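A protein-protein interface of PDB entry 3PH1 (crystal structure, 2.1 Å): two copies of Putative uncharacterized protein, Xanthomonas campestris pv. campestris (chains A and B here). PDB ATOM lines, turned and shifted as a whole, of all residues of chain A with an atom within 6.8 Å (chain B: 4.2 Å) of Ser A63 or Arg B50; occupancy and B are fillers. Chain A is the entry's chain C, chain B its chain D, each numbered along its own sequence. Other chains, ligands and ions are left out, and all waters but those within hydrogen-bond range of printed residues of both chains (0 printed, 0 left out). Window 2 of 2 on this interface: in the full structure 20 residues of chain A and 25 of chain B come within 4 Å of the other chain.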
ATOM      1  N   ARG A  59     -18.879 -28.109  27.815  1.00  0.00           N
ATOM      2  CA  ARG A  59     -19.608 -27.504  28.925  1.00  0.00           C
ATOM      3  C   ARG A  59     -21.111 -27.657  28.712  1.00  0.00           C
ATOM      4  O   ARG A  59     -21.556 -28.515  27.947  1.00  0.00           O
ATOM      5  CB  ARG A  59     -19.275 -26.014  29.019  1.00  0.00           C
ATOM      6  CG  ARG A  59     -19.658 -25.241  27.763  1.00  0.00           C
ATOM      7  CD  ARG A  59     -19.539 -23.739  27.947  1.00  0.00           C
ATOM      8  NE  ARG A  59     -19.918 -23.017  26.734  1.00  0.00           N
ATOM      9  CZ  ARG A  59     -19.901 -21.693  26.615  1.00  0.00           C
ATOM     10  NH1 ARG A  59     -20.260 -21.122  25.472  1.00  0.00           N
ATOM     11  NH2 ARG A  59     -19.528 -20.937  27.639  1.00  0.00           N
ATOM     12  N   SER A  60     -21.887 -26.821  29.396  1.00  0.00           N
ATOM     13  CA  SER A  60     -23.338 -26.842  29.260  1.00  0.00           C
ATOM     14  C   SER A  60     -23.731 -25.742  28.279  1.00  0.00           C
ATOM     15  O   SER A  60     -24.742 -25.062  28.458  1.00  0.00           O
ATOM     16  CB  SER A  60     -24.010 -26.598  30.613  1.00  0.00           C
ATOM     17  OG  SER A  60     -25.421 -26.661  30.495  1.00  0.00           O
ATOM     18  N   GLU A  61     -22.904 -25.583  27.246  1.00  0.00           N
ATOM     19  CA  GLU A  61     -23.092 -24.589  26.189  1.00  0.00           C
ATOM     20  C   GLU A  61     -23.447 -23.187  26.678  1.00  0.00           C
ATOM     21  O   GLU A  61     -24.039 -22.402  25.941  1.00  0.00           O
ATOM     22  CB  GLU A  61     -24.145 -25.084  25.177  1.00  0.00           C
ATOM     23  CG  GLU A  61     -25.530 -25.366  25.752  1.00  0.00           C
ATOM     24  CD  GLU A  61     -26.461 -24.168  25.681  1.00  0.00           C
ATOM     25  OE1 GLU A  61     -27.486 -24.167  26.395  1.00  0.00           O
ATOM     26  OE2 GLU A  61     -26.175 -23.235  24.903  1.00  0.00           O
ATOM     27  N   ASP A  62     -23.068 -22.866  27.912  1.00  0.00           N
ATOM     28  CA  ASP A  62     -23.359 -21.547  28.465  1.00  0.00           C
ATOM     29  C   ASP A  62     -22.133 -20.913  29.116  1.00  0.00           C
ATOM     30  O   ASP A  62     -21.338 -21.596  29.766  1.00  0.00           O
ATOM     31  CB  ASP A  62     -24.503 -21.632  29.489  1.00  0.00           C
ATOM     32  CG  ASP A  62     -24.071 -22.256  30.809  1.00  0.00           C
ATOM     33  OD1 ASP A  62     -23.278 -21.628  31.542  1.00  0.00           O
ATOM     34  OD2 ASP A  62     -24.530 -23.376  31.116  1.00  0.00           O
ATOM     35  N   SER A  63     -21.984 -19.604  28.929  1.00  0.00           N
ATOM     36  CA  SER A  63     -20.866 -18.860  29.503  1.00  0.00           C
ATOM     37  C   SER A  63     -21.318 -18.202  30.803  1.00  0.00           C
ATOM     38  O   SER A  63     -20.499 -17.730  31.595  1.00  0.00           O
ATOM     39  CB  SER A  63     -20.373 -17.789  28.526  1.00  0.00           C
ATOM     40  OG  SER A  63     -19.307 -17.042  29.091  1.00  0.00           O
ATOM     41  N   SER A  64     -22.632 -18.166  31.008  1.00  0.00           N
ATOM     42  CA  SER A  64     -23.200 -17.589  32.217  1.00  0.00           C
ATOM     43  C   SER A  64     -23.000 -18.604  33.335  1.00  0.00           C
ATOM     44  O   SER A  64     -21.885 -19.093  33.540  1.00  0.00           O
ATOM     45  CB  SER A  64     -24.693 -17.303  32.025  1.00  0.00           C
ATOM     46  OG  SER A  64     -25.259 -16.730  33.190  1.00  0.00           O
ATOM     47  N   GLU A  65     -24.078 -18.933  34.044  1.00  0.00           N
ATOM     48  CA  GLU A  65     -24.018 -19.890  35.139  1.00  0.00           C
ATOM     49  C   GLU A  65     -23.107 -19.388  36.279  1.00  0.00           C
ATOM     50  O   GLU A  65     -23.243 -19.826  37.426  1.00  0.00           O
ATOM     51  CB  GLU A  65     -23.539 -21.257  34.592  1.00  0.00           C
ATOM     52  CG  GLU A  65     -22.286 -21.869  35.240  1.00  0.00           C
ATOM     53  CD  GLU A  65     -22.542 -22.438  36.632  1.00  0.00           C
ATOM     54  OE1 GLU A  65     -23.395 -23.361  36.768  1.00  0.00           O
ATOM     55  OE2 GLU A  65     -21.883 -21.969  37.600  1.00  0.00           O
ATOM     56  N   GLU A  66     -22.204 -18.449  35.970  1.00  0.00           N
ATOM     57  CA  GLU A  66     -21.267 -17.944  36.988  1.00  0.00           C
ATOM     58  C   GLU A  66     -21.743 -16.611  37.574  1.00  0.00           C
ATOM     59  O   GLU A  66     -21.676 -16.405  38.787  1.00  0.00           O
ATOM     60  CB  GLU A  66     -19.848 -17.795  36.388  1.00  0.00           C
ATOM     61  CG  GLU A  66     -19.652 -16.636  35.371  1.00  0.00           C
ATOM     62  CD  GLU A  66     -18.270 -16.654  34.715  1.00  0.00           C
ATOM     63  OE1 GLU A  66     -17.248 -16.811  35.452  1.00  0.00           O
ATOM     64  OE2 GLU A  66     -18.193 -16.511  33.456  1.00  0.00           O
ATOM     65  N   ARG A  67     -22.228 -15.717  36.717  1.00  0.00           N
ATOM     66  CA  ARG A  67     -22.714 -14.425  37.185  1.00  0.00           C
ATOM     67  C   ARG A  67     -23.992 -14.624  37.987  1.00  0.00           C
ATOM     68  O   ARG A  67     -24.531 -13.682  38.570  1.00  0.00           O
ATOM     69  CB  ARG A  67     -22.957 -13.477  36.010  1.00  0.00           C
ATOM     70  CG  ARG A  67     -23.812 -14.036  34.890  1.00  0.00           C
ATOM     71  CD  ARG A  67     -23.949 -12.992  33.797  1.00  0.00           C
ATOM     72  NE  ARG A  67     -24.621 -13.501  32.607  1.00  0.00           N
ATOM     73  CZ  ARG A  67     -24.844 -12.777  31.514  1.00  0.00           C
ATOM     74  NH1 ARG A  67     -24.449 -11.511  31.463  1.00  0.00           N
ATOM     75  NH2 ARG A  67     -25.455 -13.320  30.470  1.00  0.00           N
ATOM     76  N   GLN A  75     -15.473 -15.897  40.194  1.00  0.00           N
ATOM     77  CA  GLN A  75     -15.335 -16.105  38.752  1.00  0.00           C
ATOM     78  C   GLN A  75     -13.913 -15.714  38.377  1.00  0.00           C
ATOM     79  O   GLN A  75     -13.273 -16.368  37.556  1.00  0.00           O
ATOM     80  CB  GLN A  75     -16.301 -15.222  37.960  1.00  0.00           C
ATOM     81  CG  GLN A  75     -17.756 -15.311  38.361  1.00  0.00           C
ATOM     82  CD  GLN A  75     -18.658 -14.490  37.446  1.00  0.00           C
ATOM     83  OE1 GLN A  75     -19.799 -14.192  37.794  1.00  0.00           O
ATOM     84  NE2 GLN A  75     -18.150 -14.131  36.262  1.00  0.00           N
ATOM     85  N   ALA A  79     -10.977 -17.982  36.718  1.00  0.00           N
ATOM     86  CA  ALA A  79     -10.284 -17.556  35.508  1.00  0.00           C
ATOM     87  C   ALA A  79      -8.776 -17.735  35.696  1.00  0.00           C
ATOM     88  O   ALA A  79      -8.086 -18.310  34.838  1.00  0.00           O
ATOM     89  CB  ALA A  79     -10.606 -16.090  35.205  1.00  0.00           C
ATOM     90  N   GLU B  46     -11.185 -20.815  23.617  1.00  0.00           N
ATOM     91  CA  GLU B  46     -12.276 -20.123  24.295  1.00  0.00           C
ATOM     92  C   GLU B  46     -11.933 -19.900  25.783  1.00  0.00           C
ATOM     93  O   GLU B  46     -12.156 -18.816  26.322  1.00  0.00           O
ATOM     94  CB  GLU B  46     -13.580 -20.926  24.176  1.00  0.00           C
ATOM     95  CG  GLU B  46     -14.786 -20.200  24.752  1.00  0.00           C
ATOM     96  CD  GLU B  46     -16.085 -20.982  24.626  1.00  0.00           C
ATOM     97  OE1 GLU B  46     -17.130 -20.450  25.079  1.00  0.00           O
ATOM     98  OE2 GLU B  46     -16.062 -22.118  24.083  1.00  0.00           O
ATOM     99  N   THR B  47     -11.387 -20.919  26.440  1.00  0.00           N
ATOM    100  CA  THR B  47     -11.035 -20.777  27.854  1.00  0.00           C
ATOM    101  C   THR B  47     -10.043 -19.634  28.048  1.00  0.00           C
ATOM    102  O   THR B  47     -10.232 -18.794  28.919  1.00  0.00           O
ATOM    103  CB  THR B  47     -10.413 -22.067  28.423  1.00  0.00           C
ATOM    104  OG1 THR B  47     -11.334 -23.144  28.254  1.00  0.00           O
ATOM    105  CG2 THR B  47     -10.097 -21.909  29.926  1.00  0.00           C
ATOM    106  N   LEU B  48      -8.994 -19.611  27.227  1.00  0.00           N
ATOM    107  CA  LEU B  48      -7.982 -18.569  27.307  1.00  0.00           C
ATOM    108  C   LEU B  48      -8.584 -17.164  27.162  1.00  0.00           C
ATOM    109  O   LEU B  48      -8.369 -16.286  28.000  1.00  0.00           O
ATOM    110  CB  LEU B  48      -6.923 -18.788  26.223  1.00  0.00           C
ATOM    111  CG  LEU B  48      -5.831 -17.722  26.115  1.00  0.00           C
ATOM    112  CD1 LEU B  48      -5.085 -17.643  27.438  1.00  0.00           C
ATOM    113  CD2 LEU B  48      -4.876 -18.055  24.963  1.00  0.00           C
ATOM    114  N   LEU B  49      -9.355 -16.964  26.100  1.00  0.00           N
ATOM    115  CA  LEU B  49      -9.951 -15.669  25.845  1.00  0.00           C
ATOM    116  C   LEU B  49     -10.887 -15.167  26.960  1.00  0.00           C
ATOM    117  O   LEU B  49     -10.742 -14.041  27.439  1.00  0.00           O
ATOM    118  CB  LEU B  49     -10.655 -15.712  24.478  1.00  0.00           C
ATOM    119  CG  LEU B  49      -9.910 -15.026  23.313  1.00  0.00           C
ATOM    120  CD1 LEU B  49      -8.403 -15.169  23.456  1.00  0.00           C
ATOM    121  CD2 LEU B  49     -10.396 -15.604  21.989  1.00  0.00           C
ATOM    122  N   ARG B  50     -11.828 -15.999  27.388  1.00  0.00           N
ATOM    123  CA  ARG B  50     -12.760 -15.604  28.438  1.00  0.00           C
ATOM    124  C   ARG B  50     -12.056 -15.372  29.775  1.00  0.00           C
ATOM    125  O   ARG B  50     -12.388 -14.445  30.506  1.00  0.00           O
ATOM    126  CB  ARG B  50     -13.844 -16.673  28.627  1.00  0.00           C
ATOM    127  CG  ARG B  50     -14.687 -16.941  27.396  1.00  0.00           C
ATOM    128  CD  ARG B  50     -15.861 -17.882  27.700  1.00  0.00           C
ATOM    129  NE  ARG B  50     -16.754 -18.024  26.546  1.00  0.00           N
ATOM    130  CZ  ARG B  50     -17.504 -17.040  26.057  1.00  0.00           C
ATOM    131  NH1 ARG B  50     -18.281 -17.254  25.002  1.00  0.00           N
ATOM    132  NH2 ARG B  50     -17.490 -15.843  26.628  1.00  0.00           N
ATOM    133  N   SER B  51     -11.090 -16.219  30.101  1.00  0.00           N
ATOM    134  CA  SER B  51     -10.372 -16.075  31.364  1.00  0.00           C
ATOM    135  C   SER B  51      -9.562 -14.797  31.346  1.00  0.00           C
ATOM    136  O   SER B  51      -9.507 -14.050  32.332  1.00  0.00           O
ATOM    137  CB  SER B  51      -9.444 -17.262  31.581  1.00  0.00           C
ATOM    138  OG  SER B  51     -10.196 -18.453  31.634  1.00  0.00           O
ATOM    139  N   LEU B  52      -8.923 -14.556  30.212  1.00  0.00           N
ATOM    140  CA  LEU B  52      -8.120 -13.364  30.046  1.00  0.00           C
ATOM    141  C   LEU B  52      -9.009 -12.150  30.297  1.00  0.00           C
ATOM    142  O   LEU B  52      -8.670 -11.277  31.091  1.00  0.00           O
ATOM    143  CB  LEU B  52      -7.550 -13.332  28.628  1.00  0.00           C
ATOM    144  CG  LEU B  52      -6.068 -12.993  28.482  1.00  0.00           C
ATOM    145  CD1 LEU B  52      -5.254 -13.654  29.599  1.00  0.00           C
ATOM    146  CD2 LEU B  52      -5.596 -13.470  27.116  1.00  0.00           C
ATOM    147  N   GLY B  53     -10.161 -12.120  29.635  1.00  0.00           N
ATOM    148  CA  GLY B  53     -11.068 -11.004  29.788  1.00  0.00           C
ATOM    149  C   GLY B  53     -11.465 -10.764  31.228  1.00  0.00           C
ATOM    150  O   GLY B  53     -11.649  -9.622  31.650  1.00  0.00           O
ATOM    151  N   GLN B  54     -11.588 -11.842  31.993  1.00  0.00           N
ATOM    152  CA  GLN B  54     -11.987 -11.726  33.381  1.00  0.00           C
ATOM    153  C   GLN B  54     -10.917 -11.071  34.258  1.00  0.00           C
ATOM    154  O   GLN B  54     -11.240 -10.268  35.130  1.00  0.00           O
ATOM    155  CB  GLN B  54     -12.370 -13.103  33.917  1.00  0.00           C
ATOM    156  CG  GLN B  54     -13.561 -13.072  34.854  1.00  0.00           C
ATOM    157  CD  GLN B  54     -14.605 -14.129  34.521  1.00  0.00           C
ATOM    158  OE1 GLN B  54     -15.608 -14.261  35.218  1.00  0.00           O
ATOM    159  NE2 GLN B  54     -14.373 -14.884  33.452  1.00  0.00           N
ATOM    160  N   GLY B 167     -19.230 -20.873  20.778  1.00  0.00           N
ATOM    161  CA  GLY B 167     -18.564 -20.364  21.969  1.00  0.00           C
ATOM    162  C   GLY B 167     -17.286 -19.583  21.700  1.00  0.00           C
ATOM    163  O   GLY B 167     -17.129 -18.435  22.154  1.00  0.00           O
ATOM    164  N   ASP B 170     -18.024 -16.251  19.886  1.00  0.00           N
ATOM    165  CA  ASP B 170     -18.520 -15.218  20.791  1.00  0.00           C
ATOM    166  C   ASP B 170     -17.390 -14.645  21.653  1.00  0.00           C
ATOM    167  O   ASP B 170     -17.285 -13.428  21.807  1.00  0.00           O
ATOM    168  CB  ASP B 170     -19.639 -15.778  21.678  1.00  0.00           C
ATOM    169  CG  ASP B 170     -19.989 -14.854  22.838  1.00  0.00           C
ATOM    170  OD1 ASP B 170     -19.437 -15.042  23.939  1.00  0.00           O
ATOM    171  OD2 ASP B 170     -20.808 -13.930  22.643  1.00  0.00           O
ATOM    172  N   ALA B 171     -16.548 -15.515  22.210  1.00  0.00           N
ATOM    173  CA  ALA B 171     -15.419 -15.067  23.043  1.00  0.00           C
ATOM    174  C   ALA B 171     -14.500 -14.133  22.242  1.00  0.00           C
ATOM    175  O   ALA B 171     -14.097 -13.066  22.717  1.00  0.00           O
ATOM    176  CB  ALA B 171     -14.628 -16.255  23.525  1.00  0.00           C
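No position is printed for both chains.
The side-chain amide nitrogen of Gln A75 is in hydrogen-bond range of the side-chain amide oxygen of Gln B54. The guanidinium group (NH1) of Arg A59 lies within salt-bridge range of the side-chain carboxylate (OE1) of Glu B46, at 3.2 Å. The side-chain hydroxyl (OG) of Ser A63 sits at hydrogen-bond distance from the guanidinium group (NH2) of Arg B50, at 3.3 Å. OE1 of Glu A66 lies close to OE1 of Gln B54 (3.0 Å).
Of chain B, only Arg B50 (3.3 Å) comes within 4 Å of Ser A63. Arg A67 touches none of the printed residues of chain B. Of the printed residues of chain B, Gln A75 touches Gln B54. Printed residues of chain B within 4 Å of Ala A79: Ser B51 and Gln B54. Of the printed residues of chain A, Arg B50 touches Ser A63. Of the printed residues of chain A, Ser B51 touches Ala A79. The nearest printed residue of chain B that does not touch Ser A63 is Asp B170 (5.4 Å).
Hydrophobic or aromatic side chains of chain A within 4 Å of the printed part of chain B: Ala A79. Among the printed residues, 7 pairs touch across the chains.
Arg A59 touches Gly B167 (NH1 to CA, 3.97 Å). Ala A79 touches Ser B51. Ala A79 touches Gln B54.
NH1 of Arg B50 is in salt-bridge range of OD1 of Asp B170 (2.7 Å). The backbone NH of Arg A67 lies close to the side-chain amide oxygen of Gln A75 (3.1 Å). The side-chain carboxylate of Glu A66 lies within hydrogen-bond range of the side-chain amide nitrogen of Gln A75 (2.9 Å). NH2 of Arg A59 lies within hydrogen-bond range of O of Asp A62 (2.9 Å). OE1 of Glu B46 is in salt-bridge range of NE of Arg B50. The backbone carbonyl oxygen (O) of Thr B47 lies within hydrogen-bond range of the side-chain hydroxyl (OG) of Ser B51 (2.7 Å).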
